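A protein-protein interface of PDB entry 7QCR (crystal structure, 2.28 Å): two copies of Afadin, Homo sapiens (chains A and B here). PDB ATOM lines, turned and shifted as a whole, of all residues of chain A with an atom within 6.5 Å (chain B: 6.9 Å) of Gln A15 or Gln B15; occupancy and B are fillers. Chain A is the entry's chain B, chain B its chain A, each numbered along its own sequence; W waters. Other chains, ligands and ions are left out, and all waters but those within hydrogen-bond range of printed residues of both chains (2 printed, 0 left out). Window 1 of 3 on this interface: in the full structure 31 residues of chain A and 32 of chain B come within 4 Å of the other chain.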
ATOM      1  N   LYS A  13      32.377 -21.100   5.665  1.00  0.00           N
ATOM      2  CA  LYS A  13      32.841 -19.777   6.011  1.00  0.00           C
ATOM      3  C   LYS A  13      31.568 -19.041   6.399  1.00  0.00           C
ATOM      4  O   LYS A  13      30.615 -18.993   5.612  1.00  0.00           O
ATOM      5  CB  LYS A  13      33.484 -19.107   4.783  1.00  0.00           C
ATOM      6  CG  LYS A  13      34.028 -17.715   5.046  1.00  0.00           C
ATOM      7  CD  LYS A  13      34.179 -16.925   3.748  1.00  0.00           C
ATOM      8  CE  LYS A  13      32.841 -16.591   3.125  1.00  0.00           C
ATOM      9  NZ  LYS A  13      32.299 -15.286   3.606  1.00  0.00           N
ATOM     10  N   LYS A  14      31.518 -18.521   7.623  1.00  0.00           N
ATOM     11  CA  LYS A  14      30.349 -17.788   8.103  1.00  0.00           C
ATOM     12  C   LYS A  14      30.020 -16.577   7.235  1.00  0.00           C
ATOM     13  O   LYS A  14      30.915 -15.973   6.647  1.00  0.00           O
ATOM     14  CB  LYS A  14      30.573 -17.308   9.535  1.00  0.00           C
ATOM     15  CG  LYS A  14      30.757 -18.431  10.522  1.00  0.00           C
ATOM     16  CD  LYS A  14      30.768 -17.867  11.921  1.00  0.00           C
ATOM     17  CE  LYS A  14      31.434 -18.793  12.890  1.00  0.00           C
ATOM     18  NZ  LYS A  14      31.689 -18.115  14.195  1.00  0.00           N
ATOM     19  N   GLN A  15      28.737 -16.203   7.191  1.00  0.00           N
ATOM     20  CA  GLN A  15      28.274 -15.048   6.442  1.00  0.00           C
ATOM     21  C   GLN A  15      27.293 -14.171   7.234  1.00  0.00           C
ATOM     22  O   GLN A  15      26.612 -14.646   8.143  1.00  0.00           O
ATOM     23  CB  GLN A  15      27.702 -15.471   5.087  1.00  0.00           C
ATOM     24  CG  GLN A  15      28.788 -15.636   4.021  1.00  0.00           C
ATOM     25  CD  GLN A  15      28.561 -16.796   3.076  1.00  0.00           C
ATOM     26  OE1 GLN A  15      29.486 -17.575   2.771  1.00  0.00           O
ATOM     27  NE2 GLN A  15      27.336 -16.919   2.569  1.00  0.00           N
ATOM     28  N   ASN A  16      27.246 -12.884   6.868  1.00  0.00           N
ATOM     29  CA  ASN A  16      26.425 -11.813   7.444  1.00  0.00           C
ATOM     30  C   ASN A  16      25.043 -11.681   6.753  1.00  0.00           C
ATOM     31  O   ASN A  16      24.872 -12.146   5.627  1.00  0.00           O
ATOM     32  CB  ASN A  16      27.177 -10.489   7.262  1.00  0.00           C
ATOM     33  CG  ASN A  16      28.135 -10.128   8.366  1.00  0.00           C
ATOM     34  OD1 ASN A  16      28.559 -10.968   9.173  1.00  0.00           O
ATOM     35  ND2 ASN A  16      28.495  -8.851   8.418  1.00  0.00           N
ATOM     36  N   GLY A  17      24.094 -11.017   7.412  1.00  0.00           N
ATOM     37  CA  GLY A  17      22.763 -10.767   6.867  1.00  0.00           C
ATOM     38  C   GLY A  17      21.783 -10.119   7.827  1.00  0.00           C
ATOM     39  O   GLY A  17      21.696 -10.514   8.987  1.00  0.00           O
ATOM     40  N   MET A  18      21.025  -9.130   7.348  1.00  0.00           N
ATOM     41  CA  MET A  18      19.988  -8.435   8.121  1.00  0.00           C
ATOM     42  C   MET A  18      18.656  -9.202   8.180  1.00  0.00           C
ATOM     43  O   MET A  18      17.800  -8.842   8.980  1.00  0.00           O
ATOM     44  CB  MET A  18      19.707  -7.061   7.506  1.00  0.00           C
ATOM     45  CG  MET A  18      20.914  -6.191   7.390  1.00  0.00           C
ATOM     46  SD  MET A  18      20.486  -4.617   6.605  1.00  0.00           S
ATOM     47  CE  MET A  18      20.166  -5.153   5.024  1.00  0.00           C
ATOM     48  N   GLY A  19      18.468 -10.199   7.315  1.00  0.00           N
ATOM     49  CA  GLY A  19      17.228 -10.958   7.265  1.00  0.00           C
ATOM     50  C   GLY A  19      16.118 -10.186   6.572  1.00  0.00           C
ATOM     51  O   GLY A  19      15.027 -10.031   7.119  1.00  0.00           O
ATOM     52  N   GLY A  43      13.053 -15.037  12.203  1.00  0.00           N
ATOM     53  CA  GLY A  43      14.217 -15.328  13.027  1.00  0.00           C
ATOM     54  C   GLY A  43      15.457 -14.508  12.729  1.00  0.00           C
ATOM     55  O   GLY A  43      16.436 -14.585  13.478  1.00  0.00           O
ATOM     56  N   GLY A  44      15.436 -13.735  11.646  1.00  0.00           N
ATOM     57  CA  GLY A  44      16.572 -12.908  11.259  1.00  0.00           C
ATOM     58  C   GLY A  44      16.738 -11.665  12.110  1.00  0.00           C
ATOM     59  O   GLY A  44      15.877 -11.370  12.941  1.00  0.00           O
ATOM     60  N   ALA A  45      17.829 -10.902  11.905  1.00  0.00           N
ATOM     61  CA  ALA A  45      18.089  -9.690  12.686  1.00  0.00           C
ATOM     62  C   ALA A  45      16.955  -8.656  12.639  1.00  0.00           C
ATOM     63  O   ALA A  45      16.616  -8.071  13.667  1.00  0.00           O
ATOM     64  CB  ALA A  45      19.404  -9.062  12.273  1.00  0.00           C
ATOM     65  N   ALA A  46      16.351  -8.447  11.463  1.00  0.00           N
ATOM     66  CA  ALA A  46      15.255  -7.484  11.328  1.00  0.00           C
ATOM     67  C   ALA A  46      13.988  -7.947  12.059  1.00  0.00           C
ATOM     68  O   ALA A  46      13.233  -7.125  12.584  1.00  0.00           O
ATOM     69  CB  ALA A  46      14.959  -7.221   9.854  1.00  0.00           C
ATOM     70  N   VAL A  48      13.993 -10.070  14.829  1.00  0.00           N
ATOM     71  CA  VAL A  48      14.233  -9.995  16.271  1.00  0.00           C
ATOM     72  C   VAL A  48      14.181  -8.533  16.772  1.00  0.00           C
ATOM     73  O   VAL A  48      13.679  -8.272  17.876  1.00  0.00           O
ATOM     74  CB  VAL A  48      15.495 -10.759  16.740  1.00  0.00           C
ATOM     75  CG1 VAL A  48      15.310 -12.257  16.580  1.00  0.00           C
ATOM     76  CG2 VAL A  48      16.731 -10.308  16.016  1.00  0.00           C
ATOM     77  N   SER A  83      29.649  -5.436  10.319  1.00  0.00           N
ATOM     78  CA  SER A  83      28.691  -6.196  11.128  1.00  0.00           C
ATOM     79  C   SER A  83      27.456  -5.376  11.526  1.00  0.00           C
ATOM     80  O   SER A  83      26.363  -5.921  11.594  1.00  0.00           O
ATOM     81  CB  SER A  83      29.368  -6.772  12.368  1.00  0.00           C
ATOM     82  OG  SER A  83      29.674  -5.762  13.316  1.00  0.00           O
ATOM     83  N   LYS B  13      22.531  -5.158  13.819  1.00  0.00           N
ATOM     84  CA  LYS B  13      23.772  -5.908  13.802  1.00  0.00           C
ATOM     85  C   LYS B  13      23.389  -7.187  13.065  1.00  0.00           C
ATOM     86  O   LYS B  13      22.471  -7.885  13.491  1.00  0.00           O
ATOM     87  CB  LYS B  13      24.258  -6.239  15.214  1.00  0.00           C
ATOM     88  CG  LYS B  13      25.592  -6.982  15.231  1.00  0.00           C
ATOM     89  CD  LYS B  13      25.795  -7.733  16.539  1.00  0.00           C
ATOM     90  CE  LYS B  13      24.818  -8.879  16.705  1.00  0.00           C
ATOM     91  NZ  LYS B  13      25.346 -10.165  16.156  1.00  0.00           N
ATOM     92  N   LYS B  14      24.025  -7.453  11.929  1.00  0.00           N
ATOM     93  CA  LYS B  14      23.744  -8.628  11.117  1.00  0.00           C
ATOM     94  C   LYS B  14      24.009  -9.910  11.891  1.00  0.00           C
ATOM     95  O   LYS B  14      24.888  -9.946  12.757  1.00  0.00           O
ATOM     96  CB  LYS B  14      24.614  -8.608   9.858  1.00  0.00           C
ATOM     97  CG  LYS B  14      24.418  -7.381   8.979  1.00  0.00           C
ATOM     98  CD  LYS B  14      25.221  -7.494   7.725  1.00  0.00           C
ATOM     99  CE  LYS B  14      25.637  -6.171   7.159  1.00  0.00           C
ATOM    100  NZ  LYS B  14      26.593  -6.357   6.034  1.00  0.00           N
ATOM    101  N   GLN B  15      23.243 -10.957  11.592  1.00  0.00           N
ATOM    102  CA  GLN B  15      23.479 -12.252  12.210  1.00  0.00           C
ATOM    103  C   GLN B  15      24.601 -12.906  11.388  1.00  0.00           C
ATOM    104  O   GLN B  15      24.424 -13.153  10.195  1.00  0.00           O
ATOM    105  CB  GLN B  15      22.219 -13.128  12.170  1.00  0.00           C
ATOM    106  CG  GLN B  15      21.154 -12.761  13.187  1.00  0.00           C
ATOM    107  CD  GLN B  15      19.911 -13.621  13.065  1.00  0.00           C
ATOM    108  OE1 GLN B  15      19.671 -14.296  12.048  1.00  0.00           O
ATOM    109  NE2 GLN B  15      19.058 -13.574  14.089  1.00  0.00           N
ATOM    110  N   ASN B  16      25.761 -13.147  12.010  1.00  0.00           N
ATOM    111  CA  ASN B  16      26.883 -13.777  11.337  1.00  0.00           C
ATOM    112  C   ASN B  16      26.917 -15.253  11.728  1.00  0.00           C
ATOM    113  O   ASN B  16      26.966 -15.585  12.918  1.00  0.00           O
ATOM    114  CB  ASN B  16      28.192 -13.071  11.700  1.00  0.00           C
ATOM    115  CG  ASN B  16      29.445 -13.751  11.211  1.00  0.00           C
ATOM    116  OD1 ASN B  16      30.130 -14.446  11.968  1.00  0.00           O
ATOM    117  ND2 ASN B  16      29.762 -13.582   9.939  1.00  0.00           N
ATOM    118  N   GLY B  17      26.878 -16.126  10.734  1.00  0.00           N
ATOM    119  CA  GLY B  17      26.900 -17.552  10.994  1.00  0.00           C
ATOM    120  C   GLY B  17      26.894 -18.440   9.774  1.00  0.00           C
ATOM    121  O   GLY B  17      27.075 -17.990   8.643  1.00  0.00           O
ATOM    122  N   MET B  18      26.695 -19.722  10.017  1.00  0.00           N
ATOM    123  CA  MET B  18      26.643 -20.747   8.981  1.00  0.00           C
ATOM    124  C   MET B  18      25.288 -20.844   8.276  1.00  0.00           C
ATOM    125  O   MET B  18      25.208 -21.504   7.256  1.00  0.00           O
ATOM    126  CB  MET B  18      26.967 -22.128   9.582  1.00  0.00           C
ATOM    127  CG  MET B  18      28.313 -22.199  10.256  1.00  0.00           C
ATOM    128  SD  MET B  18      28.544 -23.804  11.039  1.00  0.00           S
ATOM    129  CE  MET B  18      27.329 -23.742  12.280  1.00  0.00           C
ATOM    130  N   GLY B  19      24.236 -20.243   8.829  1.00  0.00           N
ATOM    131  CA  GLY B  19      22.902 -20.309   8.240  1.00  0.00           C
ATOM    132  C   GLY B  19      22.243 -21.648   8.502  1.00  0.00           C
ATOM    133  O   GLY B  19      21.782 -22.309   7.574  1.00  0.00           O
ATOM    134  N   VAL B  41      19.041 -22.281   6.397  1.00  0.00           N
ATOM    135  CA  VAL B  41      18.586 -20.921   6.100  1.00  0.00           C
ATOM    136  C   VAL B  41      18.804 -20.508   4.640  1.00  0.00           C
ATOM    137  O   VAL B  41      19.938 -20.520   4.172  1.00  0.00           O
ATOM    138  CB  VAL B  41      19.220 -19.912   7.074  1.00  0.00           C
ATOM    139  CG1 VAL B  41      18.809 -18.489   6.725  1.00  0.00           C
ATOM    140  CG2 VAL B  41      18.854 -20.257   8.519  1.00  0.00           C
ATOM    141  N   GLY B  43      19.700 -18.729   1.448  1.00  0.00           N
ATOM    142  CA  GLY B  43      20.711 -17.728   1.143  1.00  0.00           C
ATOM    143  C   GLY B  43      21.922 -17.717   2.056  1.00  0.00           C
ATOM    144  O   GLY B  43      22.884 -17.004   1.781  1.00  0.00           O
ATOM    145  N   GLY B  44      21.883 -18.491   3.139  1.00  0.00           N
ATOM    146  CA  GLY B  44      22.992 -18.565   4.089  1.00  0.00           C
ATOM    147  C   GLY B  44      24.168 -19.373   3.585  1.00  0.00           C
ATOM    148  O   GLY B  44      24.075 -20.000   2.529  1.00  0.00           O
ATOM    149  N   ALA B  45      25.275 -19.400   4.340  1.00  0.00           N
ATOM    150  CA  ALA B  45      26.472 -20.144   3.927  1.00  0.00           C
ATOM    151  C   ALA B  45      26.234 -21.631   3.652  1.00  0.00           C
ATOM    152  O   ALA B  45      26.758 -22.154   2.672  1.00  0.00           O
ATOM    153  CB  ALA B  45      27.594 -19.965   4.930  1.00  0.00           C
ATOM    154  N   ALA B  46      25.428 -22.302   4.476  1.00  0.00           N
ATOM    155  CA  ALA B  46      25.131 -23.722   4.280  1.00  0.00           C
ATOM    156  C   ALA B  46      24.280 -23.968   3.029  1.00  0.00           C
ATOM    157  O   ALA B  46      24.431 -24.999   2.365  1.00  0.00           O
ATOM    158  CB  ALA B  46      24.452 -24.304   5.509  1.00  0.00           C
ATOM    159  N   VAL B  48      24.275 -21.880   0.232  1.00  0.00           N
ATOM    160  CA  VAL B  48      25.123 -21.596  -0.938  1.00  0.00           C
ATOM    161  C   VAL B  48      26.101 -22.762  -1.198  1.00  0.00           C
ATOM    162  O   VAL B  48      26.350 -23.119  -2.350  1.00  0.00           O
ATOM    163  CB  VAL B  48      25.841 -20.207  -0.853  1.00  0.00           C
ATOM    164  CG1 VAL B  48      26.707 -19.928  -2.065  1.00  0.00           C
ATOM    165  CG2 VAL B  48      24.850 -19.066  -0.626  1.00  0.00           C
ATOM    166  N   SER B  83      36.079 -17.518  11.621  1.00  0.00           N
ATOM    167  CA  SER B  83      35.256 -17.354  10.423  1.00  0.00           C
ATOM    168  C   SER B  83      35.007 -18.673   9.692  1.00  0.00           C
ATOM    169  O   SER B  83      33.901 -18.909   9.214  1.00  0.00           O
ATOM    170  CB  SER B  83      35.873 -16.325   9.479  1.00  0.00           C
ATOM    171  OG  SER B  83      37.260 -16.540   9.280  1.00  0.00           O
HETATM  172  O   HOH W   1      24.990 -15.709   3.485  1.00  0.00           O
HETATM  173  O   HOH W   2      19.763 -12.147   9.854  1.00  0.00           O
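Water W2 lies within hydrogen-bond range of the backbone carbonyl oxygen (O) of Gly A17 (2.7 Å), the side-chain amide oxygen (OE1) of Gln B15 (3.1 Å), the backbone NH (N) of Ala A45 (3.1 Å) and the backbone NH (N) of Gly A19 (3.5 Å). Water W1 lies within hydrogen-bond range of the side-chain amide nitrogen (NE2) of Gln A15 (2.8 Å) and the backbone carbonyl oxygen (O) of Gly B43 (3.0 Å).
The backbone NH of Lys B14 is in hydrogen-bond range of the backbone carbonyl oxygen of Ser A83 (2.8 Å). The backbone carbonyl oxygen (O) of Gly A17 sits at hydrogen-bond distance from the backbone NH (N) of Gln B15 (3.1 Å). The side-chain amide nitrogen of Gln B15 is in hydrogen-bond range of the backbone carbonyl oxygen of Gly A43 (2.9 Å). ND2 of Asn B16 lies within hydrogen-bond range of OD1 of Asn A16, 3.0 Å away. The backbone carbonyl oxygen (O) of Gly B17 is in hydrogen-bond range of the backbone NH (N) of Gln A15 (2.8 Å). The backbone carbonyl oxygen (O) of Ser B83 sits at hydrogen-bond distance from the backbone NH (N) of Lys A14 (2.9 Å). The backbone carbonyl oxygen (O) of Gln A15 sits close to the backbone carbonyl oxygen (O) of Gln B15.
Gln A15 touches just these residues of chain B: Gln B15, Asn B16, Gly B17 and Ala B45. Of the printed residues of chain B, Asn A16 touches Lys B14 (3.6 Å), Gln B15 (3.7 Å) and Asn B16 (3.0 Å). Printed residues of chain B within 4 Å of Gly A44: Gln B15. Printed residues of chain B within 4 Å of Ser A83: Lys B13 and Lys B14. Gln B15 touches six residues of chain A. Printed residues of chain A within 4 Å of Asn B16: Lys A14, Gln A15 and Asn A16. Met B18 touches none of the printed residues of chain A. Gly B43 touches none of the printed residues of chain A. Of the printed residues of chain A, Ala B45 touches Lys A13 (3.2 Å) and Gln A15 (3.6 Å). The nearest residue of chain A that does not touch Gln B15 is Val A48 (4.4 Å). The nearest printed residue of chain A that does not touch Asn B16 is Gly A17 (5.3 Å).
Of the 14 printed residues of chain B, 7 touch a printed residue of chain A. Hydrophobic or aromatic side chains of chain B that line the printed part of chain A: Ala B45. Hydrophobic or aromatic side chains of chain A that line the printed part of chain B: Ala A45. Among the printed residues, 20 pairs touch across the chains.
Among the printed residues, pairs that only touch across the chains: Lys A13 with Ala B45, Lys A13 with Ser B83, Lys A14 with Asn B16, Lys A14 with Gly B17, Gln A15 with Asn B16, Gln A15 with Ala B45, Asn A16 with Lys B14, Asn A16 with Gln B15, Gly A17 with Lys B14, Gly A44 with Gln B15, Ala A45 with Lys B13, Ala A45 with Gln B15 and Ser A83 with Lys B13.
Lys A13 touches Ser B83, and with the chains exchanged Ser A83 touches Lys B13. Lys A14 touches Gly B17, and with the chains exchanged Gly A17 touches Lys B14. Gln A15 touches Asn B16, and with the chains exchanged Asn A16 touches Gln B15. Gln A15 touches Ala B45, and with the chains exchanged Ala A45 touches Gln B15.
The side-chain amide oxygen of Gln A15 sits close to the backbone carbonyl oxygen of Lys A13, at 3.4 Å.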
